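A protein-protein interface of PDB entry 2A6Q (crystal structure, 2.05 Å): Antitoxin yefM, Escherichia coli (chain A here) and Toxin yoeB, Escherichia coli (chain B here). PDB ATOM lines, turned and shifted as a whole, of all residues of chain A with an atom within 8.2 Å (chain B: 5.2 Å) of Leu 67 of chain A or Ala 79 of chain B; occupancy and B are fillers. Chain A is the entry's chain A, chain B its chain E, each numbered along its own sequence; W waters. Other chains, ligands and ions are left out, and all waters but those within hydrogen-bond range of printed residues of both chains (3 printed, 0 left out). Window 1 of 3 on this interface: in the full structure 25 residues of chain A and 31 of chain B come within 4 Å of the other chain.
NE of Arg 65 of chain B is in salt-bridge range of OE2 of Glu 53 of chain A. OD1 of Asp 12 of chain B is in salt-bridge range of NH2 of Arg 66 of chain A. The side-chain hydroxyl (OG) of Ser 70 of chain A lies within hydrogen-bond range of the backbone carbonyl oxygen (O) of Ala 78 of chain B.
O of Leu 57 of chain A is in hydrogen-bond range of ND2 of Asn 63 of chain A (3.0 Å). The backbone carbonyl oxygen of Ile 77 of chain B is in hydrogen-bond range of the side-chain hydroxyl of Ser 9 of chain B, 2.8 Å away. N of Cys 80 of chain B is in hydrogen-bond range of OD2 of Asp 12 of chain B (3.5 Å). O of Val 67 of chain B sits at hydrogen-bond distance from N of Ala 78 of chain B (2.8 Å). The backbone NH of Val 67 of chain B lies within hydrogen-bond range of the backbone carbonyl oxygen of Ala 79 of chain B.
Leu 52 of chain B touches Thr 54 of chain A (CD1 to CG2, 3.96 Å). Tyr 56 of chain A touches Arg 65 of chain B (CE2 to CZ, 3.7 Å). OD1 of Asn 63 of chain A touches O of Arg 81 of chain B (3.6 Å). Val 67 of chain B touches Leu 67 of chain A. Leu 67 of chain A touches Ala 78 of chain B. Leu 67 of chain A touches Ala 79 of chain B (CD1 to CB, 3.9 Å). Leu 52 of chain B touches Met 68 of chain A. Ile 71 of chain A touches Ala 78 of chain B (CD1 to CB, 3.3 Å). Leu 74 of chain A touches Ile 77 of chain B (CD1 to O, 3.5 Å). CD1 of Leu 74 of chain A touches CA of Ala 78 of chain B (3.6 Å).
Ala 62 of chain A touches none of the printed residues of chain B. Printed residues of chain B within 4 Å of Asn 63 of chain A: Arg 81. Of the printed residues of chain B, Arg 66 of chain A touches Asp 12 (3.0 Å). Of the printed residues of chain B, Leu 67 of chain A touches Val 67, Ala 78 and Ala 79. Printed residues of chain B within 4 Å of Ile 71 of chain A: Ala 78. Ser 73 of chain A touches none of the printed residues of chain B. Of the printed residues of chain A, Ala 78 of chain B touches Leu 67, Ser 70, Ile 71 and Leu 74. The nearest residue of chain A that does not touch Ala 79 of chain B is Ser 70 of chain A (4.6 Å). The nearest printed residue of chain B that does not touch Asn 63 of chain A is Ala 79 of chain B (5.9 Å).
Of the 21 printed residues of chain A, 10 touch a printed residue of chain B. Printed residues of chain A that touch a printed residue of chain B: Glu 53, Thr 54, Tyr 56, Asn 63, Arg 66, Leu 67, Met 68, Ser 70, Ile 71 and Leu 74. Hydrophobic or aromatic side chains of chain A within 4 Å of the printed part of chain B: Tyr 56, Leu 67, Met 68, Ile 71 and Leu 74. Printed residues of chain B that touch a printed residue of chain A: Asp 12, Leu 52, Arg 65, Val 67, Ile 77, Ala 78, Ala 79 and Arg 81. Hydrophobic or aromatic side chains of chain B within 4 Å of the printed part of chain A: Leu 52, Val 67, Ala 78 and Ala 79. Among the printed residues, 13 pairs touch across the chains. Among the printed residues, Asp or Glu carboxylates within 4 Å of a Lys or Arg side-chain nitrogen of the other chain: Glu 53 of chain A with Arg 65 of chain B and Arg 66 of chain A with Asp 12 of chain B.
Water W1 lies within hydrogen-bond range of the side-chain amide oxygen of Asn 63 of chain A (2.6 Å) and the backbone carbonyl oxygen of Arg 81 of chain B (3.2 Å). Water W3 bridges the side-chain carboxylate of Asp 12 of chain B and the guanidinium group of Arg 66 of chain A. Water W2 bridges OE1 of Glu 53 of chain A (3.2 Å) and NH2 of Arg 65 of chain B (3.5 Å).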
ATOM      1  N   GLU A  53      17.514  39.978 -32.837  1.00  0.00           N
ATOM      2  CA  GLU A  53      17.874  38.564 -32.906  1.00  0.00           C
ATOM      3  C   GLU A  53      18.780  38.161 -31.730  1.00  0.00           C
ATOM      4  O   GLU A  53      18.692  37.037 -31.219  1.00  0.00           O
ATOM      5  CB  GLU A  53      18.583  38.277 -34.229  1.00  0.00           C
ATOM      6  CG  GLU A  53      18.993  36.823 -34.432  1.00  0.00           C
ATOM      7  CD  GLU A  53      17.803  35.880 -34.523  1.00  0.00           C
ATOM      8  OE1 GLU A  53      16.652  36.341 -34.392  1.00  0.00           O
ATOM      9  OE2 GLU A  53      18.019  34.671 -34.725  1.00  0.00           O
ATOM     10  N   THR A  54      19.631  39.090 -31.295  1.00  0.00           N
ATOM     11  CA  THR A  54      20.548  38.842 -30.185  1.00  0.00           C
ATOM     12  C   THR A  54      19.759  38.750 -28.888  1.00  0.00           C
ATOM     13  O   THR A  54      19.986  37.862 -28.056  1.00  0.00           O
ATOM     14  CB  THR A  54      21.594  39.990 -30.031  1.00  0.00           C
ATOM     15  OG1 THR A  54      22.363  40.109 -31.234  1.00  0.00           O
ATOM     16  CG2 THR A  54      22.539  39.705 -28.868  1.00  0.00           C
ATOM     17  N   TYR A  56      16.671  38.020 -28.661  1.00  0.00           N
ATOM     18  CA  TYR A  56      15.828  36.830 -28.766  1.00  0.00           C
ATOM     19  C   TYR A  56      16.538  35.579 -28.259  1.00  0.00           C
ATOM     20  O   TYR A  56      15.966  34.796 -27.504  1.00  0.00           O
ATOM     21  CB  TYR A  56      15.380  36.608 -30.218  1.00  0.00           C
ATOM     22  CG  TYR A  56      14.729  35.255 -30.440  1.00  0.00           C
ATOM     23  CD1 TYR A  56      13.523  34.925 -29.813  1.00  0.00           C
ATOM     24  CD2 TYR A  56      15.353  34.278 -31.216  1.00  0.00           C
ATOM     25  CE1 TYR A  56      12.959  33.647 -29.951  1.00  0.00           C
ATOM     26  CE2 TYR A  56      14.809  33.006 -31.352  1.00  0.00           C
ATOM     27  CZ  TYR A  56      13.612  32.694 -30.715  1.00  0.00           C
ATOM     28  OH  TYR A  56      13.096  31.422 -30.811  1.00  0.00           O
ATOM     29  N   LEU A  57      17.792  35.404 -28.667  1.00  0.00           N
ATOM     30  CA  LEU A  57      18.576  34.238 -28.261  1.00  0.00           C
ATOM     31  C   LEU A  57      18.953  34.226 -26.786  1.00  0.00           C
ATOM     32  O   LEU A  57      19.261  33.173 -26.228  1.00  0.00           O
ATOM     33  CB  LEU A  57      19.847  34.142 -29.106  1.00  0.00           C
ATOM     34  CG  LEU A  57      19.609  33.850 -30.587  1.00  0.00           C
ATOM     35  CD1 LEU A  57      20.871  34.097 -31.381  1.00  0.00           C
ATOM     36  CD2 LEU A  57      19.134  32.423 -30.747  1.00  0.00           C
ATOM     37  N   LEU A  58      18.908  35.384 -26.144  1.00  0.00           N
ATOM     38  CA  LEU A  58      19.289  35.465 -24.738  1.00  0.00           C
ATOM     39  C   LEU A  58      18.106  35.654 -23.806  1.00  0.00           C
ATOM     40  O   LEU A  58      18.245  35.548 -22.590  1.00  0.00           O
ATOM     41  CB  LEU A  58      20.278  36.613 -24.541  1.00  0.00           C
ATOM     42  CG  LEU A  58      21.571  36.503 -25.359  1.00  0.00           C
ATOM     43  CD1 LEU A  58      22.420  37.751 -25.134  1.00  0.00           C
ATOM     44  CD2 LEU A  58      22.331  35.259 -24.957  1.00  0.00           C
ATOM     45  N   ARG A  59      16.947  35.935 -24.385  1.00  0.00           N
ATOM     46  CA  ARG A  59      15.735  36.168 -23.614  1.00  0.00           C
ATOM     47  C   ARG A  59      15.407  34.978 -22.711  1.00  0.00           C
ATOM     48  O   ARG A  59      15.043  35.144 -21.547  1.00  0.00           O
ATOM     49  CB  ARG A  59      14.584  36.450 -24.584  1.00  0.00           C
ATOM     50  CG  ARG A  59      13.636  37.555 -24.142  1.00  0.00           C
ATOM     51  CD  ARG A  59      12.845  38.073 -25.335  1.00  0.00           C
ATOM     52  NE  ARG A  59      13.336  39.367 -25.812  1.00  0.00           N
ATOM     53  CZ  ARG A  59      13.306  39.754 -27.084  1.00  0.00           C
ATOM     54  NH1 ARG A  59      12.815  38.949 -28.014  1.00  0.00           N
ATOM     55  NH2 ARG A  59      13.762  40.949 -27.428  1.00  0.00           N
ATOM     56  N   SER A  60      15.541  33.774 -23.257  1.00  0.00           N
ATOM     57  CA  SER A  60      15.266  32.557 -22.504  1.00  0.00           C
ATOM     58  C   SER A  60      16.498  32.167 -21.680  1.00  0.00           C
ATOM     59  O   SER A  60      17.527  31.815 -22.242  1.00  0.00           O
ATOM     60  CB  SER A  60      14.906  31.426 -23.475  1.00  0.00           C
ATOM     61  OG  SER A  60      14.640  30.228 -22.778  1.00  0.00           O
ATOM     62  N   PRO A  61      16.406  32.231 -20.338  1.00  0.00           N
ATOM     63  CA  PRO A  61      17.538  31.878 -19.473  1.00  0.00           C
ATOM     64  C   PRO A  61      18.190  30.543 -19.824  1.00  0.00           C
ATOM     65  O   PRO A  61      19.419  30.437 -19.868  1.00  0.00           O
ATOM     66  CB  PRO A  61      16.917  31.863 -18.081  1.00  0.00           C
ATOM     67  CG  PRO A  61      15.877  32.948 -18.177  1.00  0.00           C
ATOM     68  CD  PRO A  61      15.245  32.647 -19.528  1.00  0.00           C
ATOM     69  N   ALA A  62      17.369  29.528 -20.080  1.00  0.00           N
ATOM     70  CA  ALA A  62      17.888  28.208 -20.420  1.00  0.00           C
ATOM     71  C   ALA A  62      18.707  28.229 -21.708  1.00  0.00           C
ATOM     72  O   ALA A  62      19.744  27.571 -21.807  1.00  0.00           O
ATOM     73  CB  ALA A  62      16.741  27.207 -20.545  1.00  0.00           C
ATOM     74  N   ASN A  63      18.244  28.981 -22.699  1.00  0.00           N
ATOM     75  CA  ASN A  63      18.957  29.065 -23.966  1.00  0.00           C
ATOM     76  C   ASN A  63      20.219  29.927 -23.850  1.00  0.00           C
ATOM     77  O   ASN A  63      21.234  29.637 -24.481  1.00  0.00           O
ATOM     78  CB  ASN A  63      18.059  29.665 -25.046  1.00  0.00           C
ATOM     79  CG  ASN A  63      18.541  29.334 -26.434  1.00  0.00           C
ATOM     80  OD1 ASN A  63      18.501  28.175 -26.847  1.00  0.00           O
ATOM     81  ND2 ASN A  63      19.012  30.345 -27.163  1.00  0.00           N
ATOM     82  N   ALA A  64      20.134  31.001 -23.070  1.00  0.00           N
ATOM     83  CA  ALA A  64      21.274  31.902 -22.881  1.00  0.00           C
ATOM     84  C   ALA A  64      22.416  31.140 -22.228  1.00  0.00           C
ATOM     85  O   ALA A  64      23.580  31.257 -22.637  1.00  0.00           O
ATOM     86  CB  ALA A  64      20.874  33.092 -22.007  1.00  0.00           C
ATOM     87  N   ARG A  65      22.073  30.353 -21.213  1.00  0.00           N
ATOM     88  CA  ARG A  65      23.061  29.556 -20.499  1.00  0.00           C
ATOM     89  C   ARG A  65      23.798  28.608 -21.446  1.00  0.00           C
ATOM     90  O   ARG A  65      25.023  28.635 -21.517  1.00  0.00           O
ATOM     91  CB  ARG A  65      22.387  28.754 -19.380  1.00  0.00           C
ATOM     92  CG  ARG A  65      23.346  27.859 -18.607  1.00  0.00           C
ATOM     93  CD  ARG A  65      22.630  27.060 -17.526  1.00  0.00           C
ATOM     94  NE  ARG A  65      23.565  26.252 -16.744  1.00  0.00           N
ATOM     95  CZ  ARG A  65      23.213  25.439 -15.751  1.00  0.00           C
ATOM     96  NH1 ARG A  65      21.936  25.314 -15.406  1.00  0.00           N
ATOM     97  NH2 ARG A  65      24.141  24.751 -15.097  1.00  0.00           N
ATOM     98  N   ARG A  66      23.051  27.779 -22.171  1.00  0.00           N
ATOM     99  CA  ARG A  66      23.637  26.820 -23.113  1.00  0.00           C
ATOM    100  C   ARG A  66      24.468  27.477 -24.188  1.00  0.00           C
ATOM    101  O   ARG A  66      25.548  26.996 -24.534  1.00  0.00           O
ATOM    102  CB  ARG A  66      22.555  25.989 -23.814  1.00  0.00           C
ATOM    103  CG  ARG A  66      22.006  24.826 -23.022  1.00  0.00           C
ATOM    104  CD  ARG A  66      20.921  24.119 -23.837  1.00  0.00           C
ATOM    105  NE  ARG A  66      21.459  23.325 -24.943  1.00  0.00           N
ATOM    106  CZ  ARG A  66      21.975  22.108 -24.799  1.00  0.00           C
ATOM    107  NH1 ARG A  66      22.023  21.553 -23.597  1.00  0.00           N
ATOM    108  NH2 ARG A  66      22.426  21.441 -25.850  1.00  0.00           N
ATOM    109  N   LEU A  67      23.941  28.559 -24.745  1.00  0.00           N
ATOM    110  CA  LEU A  67      24.630  29.270 -25.799  1.00  0.00           C
ATOM    111  C   LEU A  67      25.926  29.874 -25.267  1.00  0.00           C
ATOM    112  O   LEU A  67      26.926  29.911 -25.970  1.00  0.00           O
ATOM    113  CB  LEU A  67      23.717  30.360 -26.373  1.00  0.00           C
ATOM    114  CG  LEU A  67      24.034  30.932 -27.756  1.00  0.00           C
ATOM    115  CD1 LEU A  67      24.199  29.797 -28.757  1.00  0.00           C
ATOM    116  CD2 LEU A  67      22.909  31.882 -28.187  1.00  0.00           C
ATOM    117  N   MET A  68      25.921  30.333 -24.020  1.00  0.00           N
ATOM    118  CA  MET A  68      27.131  30.924 -23.463  1.00  0.00           C
ATOM    119  C   MET A  68      28.192  29.849 -23.201  1.00  0.00           C
ATOM    120  O   MET A  68      29.382  30.068 -23.461  1.00  0.00           O
ATOM    121  CB  MET A  68      26.810  31.698 -22.185  1.00  0.00           C
ATOM    122  CG  MET A  68      27.250  33.162 -22.234  1.00  0.00           C
ATOM    123  SD  MET A  68      26.635  34.081 -23.682  1.00  0.00           S
ATOM    124  CE  MET A  68      28.025  33.903 -24.822  1.00  0.00           C
ATOM    125  N   ASP A  69      27.767  28.693 -22.693  1.00  0.00           N
ATOM    126  CA  ASP A  69      28.702  27.598 -22.444  1.00  0.00           C
ATOM    127  C   ASP A  69      29.248  27.106 -23.779  1.00  0.00           C
ATOM    128  O   ASP A  69      30.440  26.834 -23.913  1.00  0.00           O
ATOM    129  CB  ASP A  69      28.025  26.423 -21.727  1.00  0.00           C
ATOM    130  CG  ASP A  69      27.676  26.737 -20.296  1.00  0.00           C
ATOM    131  OD1 ASP A  69      28.412  27.522 -19.664  1.00  0.00           O
ATOM    132  OD2 ASP A  69      26.675  26.187 -19.794  1.00  0.00           O
ATOM    133  N   SER A  70      28.362  27.002 -24.764  1.00  0.00           N
ATOM    134  CA  SER A  70      28.728  26.541 -26.100  1.00  0.00           C
ATOM    135  C   SER A  70      29.741  27.475 -26.777  1.00  0.00           C
ATOM    136  O   SER A  70      30.730  27.011 -27.354  1.00  0.00           O
ATOM    137  CB  SER A  70      27.461  26.408 -26.964  1.00  0.00           C
ATOM    138  OG  SER A  70      27.756  25.920 -28.264  1.00  0.00           O
ATOM    139  N   ILE A  71      29.497  28.784 -26.700  1.00  0.00           N
ATOM    140  CA  ILE A  71      30.398  29.770 -27.302  1.00  0.00           C
ATOM    141  C   ILE A  71      31.745  29.735 -26.575  1.00  0.00           C
ATOM    142  O   ILE A  71      32.798  29.789 -27.202  1.00  0.00           O
ATOM    143  CB  ILE A  71      29.828  31.214 -27.200  1.00  0.00           C
ATOM    144  CG1 ILE A  71      28.457  31.299 -27.876  1.00  0.00           C
ATOM    145  CG2 ILE A  71      30.779  32.200 -27.849  1.00  0.00           C
ATOM    146  CD1 ILE A  71      28.467  30.972 -29.334  1.00  0.00           C
ATOM    147  N   ASP A  72      31.696  29.659 -25.251  1.00  0.00           N
ATOM    148  CA  ASP A  72      32.908  29.604 -24.443  1.00  0.00           C
ATOM    149  C   ASP A  72      33.803  28.473 -24.936  1.00  0.00           C
ATOM    150  O   ASP A  72      34.967  28.695 -25.271  1.00  0.00           O
ATOM    151  CB  ASP A  72      32.553  29.381 -22.971  1.00  0.00           C
ATOM    152  CG  ASP A  72      32.144  30.661 -22.265  1.00  0.00           C
ATOM    153  OD1 ASP A  72      31.740  31.626 -22.956  1.00  0.00           O
ATOM    154  OD2 ASP A  72      32.216  30.697 -21.015  1.00  0.00           O
ATOM    155  N   SER A  73      33.248  27.265 -24.991  1.00  0.00           N
ATOM    156  CA  SER A  73      33.991  26.099 -25.452  1.00  0.00           C
ATOM    157  C   SER A  73      34.592  26.326 -26.832  1.00  0.00           C
ATOM    158  O   SER A  73      35.798  26.162 -27.026  1.00  0.00           O
ATOM    159  CB  SER A  73      33.083  24.866 -25.498  1.00  0.00           C
ATOM    160  OG  SER A  73      32.563  24.573 -24.214  1.00  0.00           O
ATOM    161  N   LEU A  74      33.744  26.702 -27.785  1.00  0.00           N
ATOM    162  CA  LEU A  74      34.168  26.942 -29.160  1.00  0.00           C
ATOM    163  C   LEU A  74      35.326  27.930 -29.283  1.00  0.00           C
ATOM    164  O   LEU A  74      36.282  27.685 -30.021  1.00  0.00           O
ATOM    165  CB  LEU A  74      32.977  27.425 -29.996  1.00  0.00           C
ATOM    166  CG  LEU A  74      31.894  26.371 -30.264  1.00  0.00           C
ATOM    167  CD1 LEU A  74      30.672  27.018 -30.920  1.00  0.00           C
ATOM    168  CD2 LEU A  74      32.470  25.278 -31.159  1.00  0.00           C
ATOM    169  N   SER B   9      25.672  21.943 -29.016  1.00  0.00           N
ATOM    170  CA  SER B   9      25.149  21.866 -30.378  1.00  0.00           C
ATOM    171  C   SER B   9      25.128  20.450 -30.912  1.00  0.00           C
ATOM    172  O   SER B   9      24.294  20.106 -31.761  1.00  0.00           O
ATOM    173  CB  SER B   9      25.941  22.781 -31.328  1.00  0.00           C
ATOM    174  OG  SER B   9      27.248  22.299 -31.608  1.00  0.00           O
ATOM    175  N   ASP B  12      22.124  18.909 -29.418  1.00  0.00           N
ATOM    176  CA  ASP B  12      20.981  19.485 -30.132  1.00  0.00           C
ATOM    177  C   ASP B  12      20.774  18.708 -31.430  1.00  0.00           C
ATOM    178  O   ASP B  12      19.686  18.209 -31.706  1.00  0.00           O
ATOM    179  CB  ASP B  12      21.219  20.963 -30.494  1.00  0.00           C
ATOM    180  CG  ASP B  12      21.152  21.898 -29.301  1.00  0.00           C
ATOM    181  OD1 ASP B  12      20.627  21.503 -28.228  1.00  0.00           O
ATOM    182  OD2 ASP B  12      21.614  23.059 -29.456  1.00  0.00           O
ATOM    183  N   LEU B  52      27.647  38.220 -27.819  1.00  0.00           N
ATOM    184  CA  LEU B  52      27.561  37.259 -28.923  1.00  0.00           C
ATOM    185  C   LEU B  52      28.294  37.742 -30.173  1.00  0.00           C
ATOM    186  O   LEU B  52      28.200  37.123 -31.228  1.00  0.00           O
ATOM    187  CB  LEU B  52      26.098  36.983 -29.290  1.00  0.00           C
ATOM    188  CG  LEU B  52      25.229  36.266 -28.256  1.00  0.00           C
ATOM    189  CD1 LEU B  52      23.850  35.967 -28.855  1.00  0.00           C
ATOM    190  CD2 LEU B  52      25.910  34.970 -27.831  1.00  0.00           C
ATOM    191  N   ARG B  65      17.108  28.215 -34.110  1.00  0.00           N
ATOM    192  CA  ARG B  65      18.132  28.919 -34.868  1.00  0.00           C
ATOM    193  C   ARG B  65      19.457  28.169 -34.915  1.00  0.00           C
ATOM    194  O   ARG B  65      19.852  27.496 -33.953  1.00  0.00           O
ATOM    195  CB  ARG B  65      18.402  30.289 -34.238  1.00  0.00           C
ATOM    196  CG  ARG B  65      17.193  31.205 -34.109  1.00  0.00           C
ATOM    197  CD  ARG B  65      16.769  31.779 -35.449  1.00  0.00           C
ATOM    198  NE  ARG B  65      16.023  33.015 -35.237  1.00  0.00           N
ATOM    199  CZ  ARG B  65      14.714  33.085 -35.014  1.00  0.00           C
ATOM    200  NH1 ARG B  65      13.976  31.982 -34.987  1.00  0.00           N
ATOM    201  NH2 ARG B  65      14.151  34.267 -34.782  1.00  0.00           N
ATOM    202  N   LEU B  66      20.138  28.301 -36.045  1.00  0.00           N
ATOM    203  CA  LEU B  66      21.449  27.709 -36.227  1.00  0.00           C
ATOM    204  C   LEU B  66      22.371  28.882 -35.881  1.00  0.00           C
ATOM    205  O   LEU B  66      22.429  29.869 -36.619  1.00  0.00           O
ATOM    206  CB  LEU B  66      21.652  27.281 -37.686  1.00  0.00           C
ATOM    207  CG  LEU B  66      23.049  26.758 -38.060  1.00  0.00           C
ATOM    208  CD1 LEU B  66      23.292  25.419 -37.392  1.00  0.00           C
ATOM    209  CD2 LEU B  66      23.166  26.612 -39.566  1.00  0.00           C
ATOM    210  N   VAL B  67      23.046  28.795 -34.738  1.00  0.00           N
ATOM    211  CA  VAL B  67      23.957  29.848 -34.308  1.00  0.00           C
ATOM    212  C   VAL B  67      25.371  29.379 -34.632  1.00  0.00           C
ATOM    213  O   VAL B  67      25.728  28.228 -34.367  1.00  0.00           O
ATOM    214  CB  VAL B  67      23.812  30.117 -32.799  1.00  0.00           C
ATOM    215  CG1 VAL B  67      24.684  31.305 -32.387  1.00  0.00           C
ATOM    216  CG2 VAL B  67      22.340  30.397 -32.473  1.00  0.00           C
ATOM    217  N   ILE B  77      29.733  25.647 -34.884  1.00  0.00           N
ATOM    218  CA  ILE B  77      28.306  25.573 -34.597  1.00  0.00           C
ATOM    219  C   ILE B  77      28.034  25.669 -33.099  1.00  0.00           C
ATOM    220  O   ILE B  77      28.391  24.776 -32.326  1.00  0.00           O
ATOM    221  CB  ILE B  77      27.721  24.273 -35.167  1.00  0.00           C
ATOM    222  CG1 ILE B  77      27.971  24.241 -36.677  1.00  0.00           C
ATOM    223  CG2 ILE B  77      26.216  24.190 -34.886  1.00  0.00           C
ATOM    224  CD1 ILE B  77      27.525  22.959 -37.346  1.00  0.00           C
ATOM    225  N   ALA B  78      27.424  26.780 -32.696  1.00  0.00           N
ATOM    226  CA  ALA B  78      27.095  27.021 -31.299  1.00  0.00           C
ATOM    227  C   ALA B  78      25.748  26.420 -30.900  1.00  0.00           C
ATOM    228  O   ALA B  78      25.525  26.103 -29.728  1.00  0.00           O
ATOM    229  CB  ALA B  78      27.084  28.511 -31.029  1.00  0.00           C
ATOM    230  N   ALA B  79      24.840  26.275 -31.862  1.00  0.00           N
ATOM    231  CA  ALA B  79      23.530  25.711 -31.548  1.00  0.00           C
ATOM    232  C   ALA B  79      22.668  25.428 -32.767  1.00  0.00           C
ATOM    233  O   ALA B  79      22.877  25.989 -33.847  1.00  0.00           O
ATOM    234  CB  ALA B  79      22.777  26.648 -30.593  1.00  0.00           C
ATOM    235  N   CYS B  80      21.696  24.537 -32.586  1.00  0.00           N
ATOM    236  CA  CYS B  80      20.758  24.206 -33.654  1.00  0.00           C
ATOM    237  C   CYS B  80      19.395  23.860 -33.056  1.00  0.00           C
ATOM    238  O   CYS B  80      18.578  23.194 -33.683  1.00  0.00           O
ATOM    239  CB  CYS B  80      21.293  23.064 -34.531  1.00  0.00           C
ATOM    240  SG  CYS B  80      21.433  21.447 -33.770  1.00  0.00           S
ATOM    241  N   ARG B  81      19.162  24.341 -31.834  1.00  0.00           N
ATOM    242  CA  ARG B  81      17.902  24.139 -31.114  1.00  0.00           C
ATOM    243  C   ARG B  81      17.756  25.284 -30.102  1.00  0.00           C
ATOM    244  O   ARG B  81      18.758  25.744 -29.541  1.00  0.00           O
ATOM    245  CB  ARG B  81      17.922  22.786 -30.381  1.00  0.00           C
ATOM    246  CG  ARG B  81      16.660  22.458 -29.585  1.00  0.00           C
ATOM    247  CD  ARG B  81      16.808  21.150 -28.811  1.00  0.00           C
ATOM    248  NE  ARG B  81      15.596  20.801 -28.070  1.00  0.00           N
ATOM    249  CZ  ARG B  81      15.517  19.813 -27.181  1.00  0.00           C
ATOM    250  NH1 ARG B  81      16.580  19.063 -26.905  1.00  0.00           N
ATOM    251  NH2 ARG B  81      14.368  19.568 -26.565  1.00  0.00           N
HETATM  252  O   HOH W   1      20.862  27.254 -27.580  1.00  0.00           O
HETATM  253  O   HOH W   2      15.858  35.705 -37.423  1.00  0.00           O
HETATM  254  O   HOH W   3      21.799  24.716 -27.393  1.00  0.00           O
